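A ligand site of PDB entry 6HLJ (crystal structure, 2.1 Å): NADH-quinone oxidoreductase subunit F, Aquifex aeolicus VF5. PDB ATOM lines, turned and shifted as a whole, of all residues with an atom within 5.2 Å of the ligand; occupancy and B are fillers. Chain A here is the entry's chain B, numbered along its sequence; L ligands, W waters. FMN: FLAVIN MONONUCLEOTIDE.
The backbone carbonyl oxygen of Asn 219 is in hydrogen-bond range of the backbone NH of Asn 92, 2.8 Å away. The backbone carbonyl oxygen of Asp 94 sits at hydrogen-bond distance from the side-chain hydroxyl of Ser 96 (2.7 Å). OE2 of Glu 95 sits at hydrogen-bond distance from N of Asp 103, at 2.8 Å. N of Gly 65 sits at hydrogen-bond distance from O of Phe 71, 2.9 Å away. The side-chain amino group (NZ) of Lys 76 lies within hydrogen-bond range of the backbone carbonyl oxygen (O) of Val 218 (2.7 Å). The backbone NH of Leu 395 lies close to the side-chain sulfur of Cys 393 (3.5 Å). The side-chain amide nitrogen of Asn 220 is in hydrogen-bond range of the side-chain carboxylate of Asp 103, at 2.7 Å. OD1 of Asn 92 is in hydrogen-bond range of N of Asp 94 (3.1 Å).
O of Gly 183 sits close to O2' of the ligand, at 3.5 Å. The side-chain amide nitrogen (ND2) of Asn 219 is in hydrogen-bond range of an oxygen (O3P) of the ligand (3.0 Å). The side-chain amide nitrogen of Asn 220 sits at hydrogen-bond distance from an oxygen (O2) of the ligand (2.8 Å). NZ of Lys 76 is in salt-bridge range of O2P of the ligand, at 2.8 Å. O2' of the ligand lies within hydrogen-bond range of N of Glu 185 (2.9 Å). An oxygen (O4) of the ligand lies within hydrogen-bond range of the backbone NH of Glu 95 (3.1 Å). N of Gly 67 sits at hydrogen-bond distance from O1P of the ligand. The backbone NH (N) of Arg 66 sits at hydrogen-bond distance from an oxygen (O1P) of the ligand (3.2 Å). An oxygen (O3P) of the ligand lies within hydrogen-bond range of the side-chain hydroxyl (OG1) of Thr 223, at 2.6 Å. The backbone NH (N) of Asn 220 lies within hydrogen-bond range of an oxygen (O3P) of the ligand, 2.9 Å away. ND2 of Asn 92 sits at hydrogen-bond distance from O4' of the ligand (3.0 Å).
Water W9 lies within hydrogen-bond range of O1P of the ligand (2.7 Å), N of Ala 69 (2.8 Å) and N of Gly 68 (3.3 Å). Water W7 lies within hydrogen-bond range of O4 of the ligand (2.7 Å) and N of Ser 96 (2.9 Å). Water W4 lies within hydrogen-bond range of an oxygen (O2P) of the ligand (2.7 Å), the backbone carbonyl oxygen (O) of Phe 71 (2.8 Å), the side-chain hydroxyl (OG1) of Thr 73 (2.8 Å), the side-chain amide nitrogen (ND2) of Asn 219 (3.2 Å) and the backbone NH (N) of Gly 65 (3.4 Å). Water W2 lies within hydrogen-bond range of an oxygen (O2P) of the ligand (2.7 Å), the backbone NH of Phe 71 (2.8 Å) and the backbone NH of Gly 70 (3.3 Å). Water W5 lies within hydrogen-bond range of OH of Tyr 180 (2.8 Å) and N5 of the ligand (3.4 Å).
The backbone carbonyl oxygen (O) of Val 218 lies close to an oxygen (O5') of the ligand (3.4 Å). Gly 65 touches the ligand (CA to O1P, 3.2 Å). Asp 94 touches the ligand (C to O4, 3.3 Å). Ser 96 touches the ligand (N to O4, 3.9 Å). CE2 of Tyr 180 touches C7M of the ligand, 3.6 Å away. Ile 181 touches the ligand. Glu 184 touches the ligand (CA to O2', 3.6 Å). Gly 394 touches the ligand. Leu 395 touches the ligand. Hydrophobic or aromatic side chains that line the ligand: Tyr 180, Ile 181, Val 218 and Leu 395. Along chain A the residues within 4 Å of the ligand span positions 65 to 395.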
ATOM      1  N   GLY A  65      26.786  -9.122 -10.946  1.00  0.00           N
ATOM      2  CA  GLY A  65      26.010  -8.948 -12.158  1.00  0.00           C
ATOM      3  C   GLY A  65      25.111 -10.133 -12.468  1.00  0.00           C
ATOM      4  O   GLY A  65      25.545 -11.279 -12.318  1.00  0.00           O
ATOM      5  N   ARG A  66      23.858  -9.858 -12.838  1.00  0.00           N
ATOM      6  CA  ARG A  66      22.833 -10.871 -13.167  1.00  0.00           C
ATOM      7  C   ARG A  66      22.659 -11.066 -14.680  1.00  0.00           C
ATOM      8  O   ARG A  66      21.784 -11.823 -15.110  1.00  0.00           O
ATOM      9  CB  ARG A  66      21.468 -10.462 -12.540  1.00  0.00           C
ATOM     10  CG  ARG A  66      21.391 -10.406 -11.019  1.00  0.00           C
ATOM     11  CD  ARG A  66      21.825 -11.679 -10.350  1.00  0.00           C
ATOM     12  NE  ARG A  66      21.380 -11.732  -8.945  1.00  0.00           N
ATOM     13  CZ  ARG A  66      22.196 -11.696  -7.899  1.00  0.00           C
ATOM     14  NH1 ARG A  66      21.697 -11.760  -6.678  1.00  0.00           N
ATOM     15  NH2 ARG A  66      23.508 -11.606  -8.074  1.00  0.00           N
ATOM     16  N   GLY A  67      23.496 -10.377 -15.459  1.00  0.00           N
ATOM     17  CA  GLY A  67      23.467 -10.409 -16.914  1.00  0.00           C
ATOM     18  C   GLY A  67      24.247 -11.533 -17.567  1.00  0.00           C
ATOM     19  O   GLY A  67      24.217 -11.636 -18.788  1.00  0.00           O
ATOM     20  N   GLY A  68      24.933 -12.367 -16.786  1.00  0.00           N
ATOM     21  CA  GLY A  68      25.669 -13.522 -17.312  1.00  0.00           C
ATOM     22  C   GLY A  68      27.149 -13.590 -16.997  1.00  0.00           C
ATOM     23  O   GLY A  68      27.701 -14.694 -16.955  1.00  0.00           O
ATOM     24  N   ALA A  69      27.838 -12.434 -16.822  1.00  0.00           N
ATOM     25  CA  ALA A  69      29.288 -12.383 -16.581  1.00  0.00           C
ATOM     26  C   ALA A  69      29.649 -12.345 -15.108  1.00  0.00           C
ATOM     27  O   ALA A  69      30.808 -12.558 -14.774  1.00  0.00           O
ATOM     28  CB  ALA A  69      29.916 -11.204 -17.315  1.00  0.00           C
ATOM     29  N   GLY A  70      28.679 -12.027 -14.237  1.00  0.00           N
ATOM     30  CA  GLY A  70      28.846 -12.027 -12.794  1.00  0.00           C
ATOM     31  C   GLY A  70      29.951 -11.150 -12.231  1.00  0.00           C
ATOM     32  O   GLY A  70      30.581 -11.522 -11.225  1.00  0.00           O
ATOM     33  N   PHE A  71      30.176  -9.965 -12.835  1.00  0.00           N
ATOM     34  CA  PHE A  71      31.184  -9.059 -12.277  1.00  0.00           C
ATOM     35  C   PHE A  71      30.638  -8.420 -10.976  1.00  0.00           C
ATOM     36  O   PHE A  71      29.473  -8.008 -10.967  1.00  0.00           O
ATOM     37  CB  PHE A  71      31.608  -7.970 -13.298  1.00  0.00           C
ATOM     38  CG  PHE A  71      32.891  -7.274 -12.907  1.00  0.00           C
ATOM     39  CD1 PHE A  71      32.861  -6.119 -12.127  1.00  0.00           C
ATOM     40  CD2 PHE A  71      34.124  -7.776 -13.297  1.00  0.00           C
ATOM     41  CE1 PHE A  71      34.051  -5.505 -11.728  1.00  0.00           C
ATOM     42  CE2 PHE A  71      35.310  -7.148 -12.917  1.00  0.00           C
ATOM     43  CZ  PHE A  71      35.267  -6.012 -12.118  1.00  0.00           C
ATOM     44  N   THR A  73      29.224  -5.909  -8.726  1.00  0.00           N
ATOM     45  CA  THR A  73      28.559  -4.631  -9.023  1.00  0.00           C
ATOM     46  C   THR A  73      29.218  -3.434  -8.362  1.00  0.00           C
ATOM     47  O   THR A  73      29.490  -2.445  -9.031  1.00  0.00           O
ATOM     48  CB  THR A  73      27.084  -4.749  -8.700  1.00  0.00           C
ATOM     49  OG1 THR A  73      26.631  -5.959  -9.310  1.00  0.00           O
ATOM     50  CG2 THR A  73      26.262  -3.555  -9.222  1.00  0.00           C
ATOM     51  N   LYS A  76      32.511  -2.749 -10.015  1.00  0.00           N
ATOM     52  CA  LYS A  76      32.288  -2.124 -11.331  1.00  0.00           C
ATOM     53  C   LYS A  76      32.108  -0.601 -11.134  1.00  0.00           C
ATOM     54  O   LYS A  76      32.677   0.191 -11.876  1.00  0.00           O
ATOM     55  CB  LYS A  76      31.046  -2.715 -12.010  1.00  0.00           C
ATOM     56  CG  LYS A  76      30.970  -2.367 -13.501  1.00  0.00           C
ATOM     57  CD  LYS A  76      29.620  -2.668 -14.169  1.00  0.00           C
ATOM     58  CE  LYS A  76      29.332  -4.143 -14.283  1.00  0.00           C
ATOM     59  NZ  LYS A  76      28.422  -4.456 -15.413  1.00  0.00           N
ATOM     60  N   ASN A  92      20.452  -2.435 -18.731  1.00  0.00           N
ATOM     61  CA  ASN A  92      20.379  -3.370 -19.831  1.00  0.00           C
ATOM     62  C   ASN A  92      19.085  -4.195 -19.739  1.00  0.00           C
ATOM     63  O   ASN A  92      18.997  -5.151 -18.968  1.00  0.00           O
ATOM     64  CB  ASN A  92      21.663  -4.224 -19.902  1.00  0.00           C
ATOM     65  CG  ASN A  92      21.805  -5.076 -21.146  1.00  0.00           C
ATOM     66  OD1 ASN A  92      20.834  -5.349 -21.867  1.00  0.00           O
ATOM     67  ND2 ASN A  92      23.049  -5.496 -21.454  1.00  0.00           N
ATOM     68  N   ASP A  94      17.792  -5.663 -22.549  1.00  0.00           N
ATOM     69  CA  ASP A  94      17.775  -6.312 -23.870  1.00  0.00           C
ATOM     70  C   ASP A  94      17.372  -7.790 -23.842  1.00  0.00           C
ATOM     71  O   ASP A  94      17.124  -8.345 -24.901  1.00  0.00           O
ATOM     72  CB  ASP A  94      19.101  -6.135 -24.635  1.00  0.00           C
ATOM     73  CG  ASP A  94      18.886  -6.282 -26.138  1.00  0.00           C
ATOM     74  OD1 ASP A  94      18.162  -5.446 -26.716  1.00  0.00           O
ATOM     75  OD2 ASP A  94      19.374  -7.277 -26.714  1.00  0.00           O
ATOM     76  N   GLU A  95      17.317  -8.429 -22.656  1.00  0.00           N
ATOM     77  CA  GLU A  95      16.918  -9.835 -22.432  1.00  0.00           C
ATOM     78  C   GLU A  95      16.361 -10.557 -23.690  1.00  0.00           C
ATOM     79  O   GLU A  95      15.196 -10.350 -24.053  1.00  0.00           O
ATOM     80  CB  GLU A  95      15.913  -9.883 -21.281  1.00  0.00           C
ATOM     81  CG  GLU A  95      15.418 -11.275 -20.942  1.00  0.00           C
ATOM     82  CD  GLU A  95      14.602 -11.282 -19.674  1.00  0.00           C
ATOM     83  OE1 GLU A  95      13.466 -10.750 -19.679  1.00  0.00           O
ATOM     84  OE2 GLU A  95      15.116 -11.783 -18.658  1.00  0.00           O
ATOM     85  N   SER A  96      17.230 -11.322 -24.383  1.00  0.00           N
ATOM     86  CA  SER A  96      16.941 -12.044 -25.634  1.00  0.00           C
ATOM     87  C   SER A  96      17.512 -13.472 -25.668  1.00  0.00           C
ATOM     88  O   SER A  96      17.374 -14.164 -26.688  1.00  0.00           O
ATOM     89  CB  SER A  96      17.541 -11.299 -26.822  1.00  0.00           C
ATOM     90  OG  SER A  96      16.964 -10.034 -27.033  1.00  0.00           O
ATOM     91  N   ASP A 103      13.855 -10.788 -16.380  1.00  0.00           N
ATOM     92  CA  ASP A 103      13.858  -9.322 -16.324  1.00  0.00           C
ATOM     93  C   ASP A 103      12.539  -8.678 -16.652  1.00  0.00           C
ATOM     94  O   ASP A 103      12.163  -7.718 -15.981  1.00  0.00           O
ATOM     95  CB  ASP A 103      14.972  -8.730 -17.225  1.00  0.00           C
ATOM     96  CG  ASP A 103      16.371  -9.186 -16.831  1.00  0.00           C
ATOM     97  OD1 ASP A 103      16.525  -9.767 -15.749  1.00  0.00           O
ATOM     98  OD2 ASP A 103      17.313  -9.000 -17.658  1.00  0.00           O
ATOM     99  N   TYR A 180      20.037  -9.784 -30.938  1.00  0.00           N
ATOM    100  CA  TYR A 180      20.477 -10.299 -29.641  1.00  0.00           C
ATOM    101  C   TYR A 180      21.807  -9.700 -29.230  1.00  0.00           C
ATOM    102  O   TYR A 180      22.037  -9.467 -28.044  1.00  0.00           O
ATOM    103  CB  TYR A 180      20.558 -11.819 -29.710  1.00  0.00           C
ATOM    104  CG  TYR A 180      21.349 -12.475 -28.595  1.00  0.00           C
ATOM    105  CD1 TYR A 180      20.842 -12.524 -27.293  1.00  0.00           C
ATOM    106  CD2 TYR A 180      22.564 -13.084 -28.849  1.00  0.00           C
ATOM    107  CE1 TYR A 180      21.549 -13.135 -26.268  1.00  0.00           C
ATOM    108  CE2 TYR A 180      23.244 -13.780 -27.841  1.00  0.00           C
ATOM    109  CZ  TYR A 180      22.737 -13.785 -26.548  1.00  0.00           C
ATOM    110  OH  TYR A 180      23.421 -14.397 -25.528  1.00  0.00           O
ATOM    111  N   ILE A 181      22.675  -9.422 -30.212  1.00  0.00           N
ATOM    112  CA  ILE A 181      24.000  -8.865 -29.979  1.00  0.00           C
ATOM    113  C   ILE A 181      23.929  -7.522 -29.270  1.00  0.00           C
ATOM    114  O   ILE A 181      24.880  -7.149 -28.598  1.00  0.00           O
ATOM    115  CB  ILE A 181      24.841  -8.818 -31.299  1.00  0.00           C
ATOM    116  CG1 ILE A 181      26.339  -8.717 -31.004  1.00  0.00           C
ATOM    117  CG2 ILE A 181      24.380  -7.705 -32.268  1.00  0.00           C
ATOM    118  CD1 ILE A 181      26.905  -9.747 -29.994  1.00  0.00           C
ATOM    119  N   GLY A 183      22.580  -6.816 -26.642  1.00  0.00           N
ATOM    120  CA  GLY A 183      22.670  -7.034 -25.204  1.00  0.00           C
ATOM    121  C   GLY A 183      24.122  -6.998 -24.751  1.00  0.00           C
ATOM    122  O   GLY A 183      24.389  -6.846 -23.557  1.00  0.00           O
ATOM    123  N   GLU A 184      25.077  -7.191 -25.711  1.00  0.00           N
ATOM    124  CA  GLU A 184      26.510  -7.096 -25.428  1.00  0.00           C
ATOM    125  C   GLU A 184      26.741  -5.636 -25.084  1.00  0.00           C
ATOM    126  O   GLU A 184      26.255  -4.759 -25.806  1.00  0.00           O
ATOM    127  CB  GLU A 184      27.361  -7.541 -26.654  1.00  0.00           C
ATOM    128  CG  GLU A 184      28.791  -7.886 -26.296  1.00  0.00           C
ATOM    129  CD  GLU A 184      29.756  -6.724 -26.200  1.00  0.00           C
ATOM    130  OE1 GLU A 184      29.449  -5.644 -26.767  1.00  0.00           O
ATOM    131  OE2 GLU A 184      30.848  -6.907 -25.615  1.00  0.00           O
ATOM    132  N   GLU A 185      27.374  -5.352 -23.949  1.00  0.00           N
ATOM    133  CA  GLU A 185      27.422  -3.982 -23.422  1.00  0.00           C
ATOM    134  C   GLU A 185      28.012  -2.932 -24.394  1.00  0.00           C
ATOM    135  O   GLU A 185      27.481  -1.814 -24.436  1.00  0.00           O
ATOM    136  CB  GLU A 185      28.087  -3.903 -22.039  1.00  0.00           C
ATOM    137  CG  GLU A 185      29.536  -4.352 -21.969  1.00  0.00           C
ATOM    138  CD  GLU A 185      30.149  -4.352 -20.573  1.00  0.00           C
ATOM    139  OE1 GLU A 185      29.566  -3.740 -19.646  1.00  0.00           O
ATOM    140  OE2 GLU A 185      31.245  -4.951 -20.419  1.00  0.00           O
ATOM    141  N   VAL A 218      27.106  -0.182 -17.289  1.00  0.00           N
ATOM    142  CA  VAL A 218      25.993  -0.950 -17.829  1.00  0.00           C
ATOM    143  C   VAL A 218      25.710  -2.034 -16.786  1.00  0.00           C
ATOM    144  O   VAL A 218      26.628  -2.733 -16.378  1.00  0.00           O
ATOM    145  CB  VAL A 218      26.317  -1.565 -19.222  1.00  0.00           C
ATOM    146  CG1 VAL A 218      25.126  -2.380 -19.749  1.00  0.00           C
ATOM    147  CG2 VAL A 218      26.724  -0.502 -20.238  1.00  0.00           C
ATOM    148  N   ASN A 219      24.455  -2.137 -16.330  1.00  0.00           N
ATOM    149  CA  ASN A 219      24.022  -3.171 -15.379  1.00  0.00           C
ATOM    150  C   ASN A 219      22.710  -3.780 -15.864  1.00  0.00           C
ATOM    151  O   ASN A 219      21.902  -3.059 -16.461  1.00  0.00           O
ATOM    152  CB  ASN A 219      23.875  -2.643 -13.945  1.00  0.00           C
ATOM    153  CG  ASN A 219      25.156  -2.635 -13.143  1.00  0.00           C
ATOM    154  OD1 ASN A 219      25.566  -1.594 -12.611  1.00  0.00           O
ATOM    155  ND2 ASN A 219      25.811  -3.784 -12.984  1.00  0.00           N
ATOM    156  N   ASN A 220      22.519  -5.087 -15.623  1.00  0.00           N
ATOM    157  CA  ASN A 220      21.308  -5.827 -15.975  1.00  0.00           C
ATOM    158  C   ASN A 220      20.137  -5.389 -15.068  1.00  0.00           C
ATOM    159  O   ASN A 220      20.366  -4.988 -13.929  1.00  0.00           O
ATOM    160  CB  ASN A 220      21.577  -7.343 -15.803  1.00  0.00           C
ATOM    161  CG  ASN A 220      20.389  -8.238 -16.028  1.00  0.00           C
ATOM    162  OD1 ASN A 220      19.801  -8.763 -15.096  1.00  0.00           O
ATOM    163  ND2 ASN A 220      19.931  -8.320 -17.258  1.00  0.00           N
ATOM    164  N   VAL A 221      18.898  -5.493 -15.571  1.00  0.00           N
ATOM    165  CA  VAL A 221      17.654  -5.188 -14.851  1.00  0.00           C
ATOM    166  C   VAL A 221      17.632  -5.850 -13.491  1.00  0.00           C
ATOM    167  O   VAL A 221      17.441  -5.156 -12.488  1.00  0.00           O
ATOM    168  CB  VAL A 221      16.398  -5.638 -15.673  1.00  0.00           C
ATOM    169  CG1 VAL A 221      15.111  -5.557 -14.839  1.00  0.00           C
ATOM    170  CG2 VAL A 221      16.281  -4.813 -16.931  1.00  0.00           C
ATOM    171  N   THR A 223      20.111  -7.094 -11.674  1.00  0.00           N
ATOM    172  CA  THR A 223      21.151  -6.532 -10.787  1.00  0.00           C
ATOM    173  C   THR A 223      20.619  -5.252 -10.097  1.00  0.00           C
ATOM    174  O   THR A 223      20.636  -5.144  -8.874  1.00  0.00           O
ATOM    175  CB  THR A 223      22.422  -6.180 -11.566  1.00  0.00           C
ATOM    176  OG1 THR A 223      22.727  -7.212 -12.487  1.00  0.00           O
ATOM    177  CG2 THR A 223      23.619  -5.936 -10.633  1.00  0.00           C
ATOM    178  N   CYS A 393      33.967 -10.517 -28.938  1.00  0.00           N
ATOM    179  CA  CYS A 393      32.906 -10.516 -27.920  1.00  0.00           C
ATOM    180  C   CYS A 393      32.551 -11.963 -27.497  1.00  0.00           C
ATOM    181  O   CYS A 393      33.056 -12.907 -28.095  1.00  0.00           O
ATOM    182  CB  CYS A 393      31.695  -9.688 -28.329  1.00  0.00           C
ATOM    183  SG  CYS A 393      30.314 -10.617 -29.077  1.00  0.00           S
ATOM    184  N   GLY A 394      31.770 -12.080 -26.425  1.00  0.00           N
ATOM    185  CA  GLY A 394      31.375 -13.348 -25.824  1.00  0.00           C
ATOM    186  C   GLY A 394      30.593 -14.306 -26.710  1.00  0.00           C
ATOM    187  O   GLY A 394      30.649 -15.505 -26.474  1.00  0.00           O
ATOM    188  N   LEU A 395      29.851 -13.792 -27.704  1.00  0.00           N
ATOM    189  CA  LEU A 395      29.083 -14.643 -28.625  1.00  0.00           C
ATOM    190  C   LEU A 395      29.946 -15.702 -29.381  1.00  0.00           C
ATOM    191  O   LEU A 395      29.608 -16.891 -29.359  1.00  0.00           O
ATOM    192  CB  LEU A 395      28.241 -13.820 -29.607  1.00  0.00           C
ATOM    193  CG  LEU A 395      27.153 -14.590 -30.398  1.00  0.00           C
ATOM    194  CD1 LEU A 395      25.997 -13.664 -30.732  1.00  0.00           C
ATOM    195  CD2 LEU A 395      27.737 -15.236 -31.681  1.00  0.00           C
HETATM  196  N1  FMN L   1      23.389  -8.577 -20.391  1.00  0.00           N
HETATM  197  C2  FMN L   1      22.119  -8.222 -20.092  1.00  0.00           C
HETATM  198  O2  FMN L   1      21.884  -7.565 -19.077  1.00  0.00           O
HETATM  199  N3  FMN L   1      21.077  -8.511 -20.982  1.00  0.00           N
HETATM  200  C4  FMN L   1      21.220  -9.126 -22.222  1.00  0.00           C
HETATM  201  O4  FMN L   1      20.235  -9.273 -22.953  1.00  0.00           O
HETATM  202  C4A FMN L   1      22.609  -9.483 -22.543  1.00  0.00           C
HETATM  203  N5  FMN L   1      22.852 -10.039 -23.700  1.00  0.00           N
HETATM  204  C5A FMN L   1      24.183 -10.330 -24.016  1.00  0.00           C
HETATM  205  C6  FMN L   1      24.475 -10.873 -25.268  1.00  0.00           C
HETATM  206  C7  FMN L   1      25.783 -11.169 -25.640  1.00  0.00           C
HETATM  207  C7M FMN L   1      26.049 -11.742 -27.009  1.00  0.00           C
HETATM  208  C8  FMN L   1      26.841 -10.922 -24.728  1.00  0.00           C
HETATM  209  C8M FMN L   1      28.270 -11.318 -25.035  1.00  0.00           C
HETATM  210  C9  FMN L   1      26.550 -10.357 -23.480  1.00  0.00           C
HETATM  211  C9A FMN L   1      25.245 -10.071 -23.116  1.00  0.00           C
HETATM  212  N10 FMN L   1      24.919  -9.482 -21.863  1.00  0.00           N
HETATM  213  C10 FMN L   1      23.617  -9.170 -21.554  1.00  0.00           C
HETATM  214  C1' FMN L   1      25.986  -9.170 -20.892  1.00  0.00           C
HETATM  215  C2' FMN L   1      26.403  -7.703 -20.959  1.00  0.00           C
HETATM  216  O2' FMN L   1      27.394  -7.515 -21.967  1.00  0.00           O
HETATM  217  C3' FMN L   1      26.925  -7.217 -19.603  1.00  0.00           C
HETATM  218  O3' FMN L   1      27.808  -8.199 -19.062  1.00  0.00           O
HETATM  219  C4' FMN L   1      25.881  -6.870 -18.537  1.00  0.00           C
HETATM  220  O4' FMN L   1      24.763  -6.141 -19.073  1.00  0.00           O
HETATM  221  C5' FMN L   1      26.492  -6.091 -17.403  1.00  0.00           C
HETATM  222  O5' FMN L   1      25.541  -5.999 -16.328  1.00  0.00           O
HETATM  223  P   FMN L   1      25.627  -6.886 -14.992  1.00  0.00           P
HETATM  224  O1P FMN L   1      25.404  -8.349 -15.251  1.00  0.00           O
HETATM  225  O2P FMN L   1      27.076  -6.658 -14.412  1.00  0.00           O
HETATM  226  O3P FMN L   1      24.626  -6.290 -14.073  1.00  0.00           O
HETATM  227  O   HOH W   1      26.517 -12.455 -20.492  1.00  0.00           O
HETATM  228  O   HOH W   2      28.752  -8.752 -14.865  1.00  0.00           O
HETATM  229  O   HOH W   3      18.424  -7.667 -19.943  1.00  0.00           O
HETATM  230  O   HOH W   4      27.745  -6.039 -11.851  1.00  0.00           O
HETATM  231  O   HOH W   5      22.768 -13.407 -22.984  1.00  0.00           O
HETATM  232  O   HOH W   6      22.424 -12.168 -20.580  1.00  0.00           O
HETATM  233  O   HOH W   7      19.754 -11.927 -23.165  1.00  0.00           O
HETATM  234  O   HOH W   8      20.514  -9.463 -25.763  1.00  0.00           O
HETATM  235  O   HOH W   9      27.036  -9.779 -16.846  1.00  0.00           O
HETATM  236  O   HOH W  10      29.927  -9.259 -22.040  1.00  0.00           O
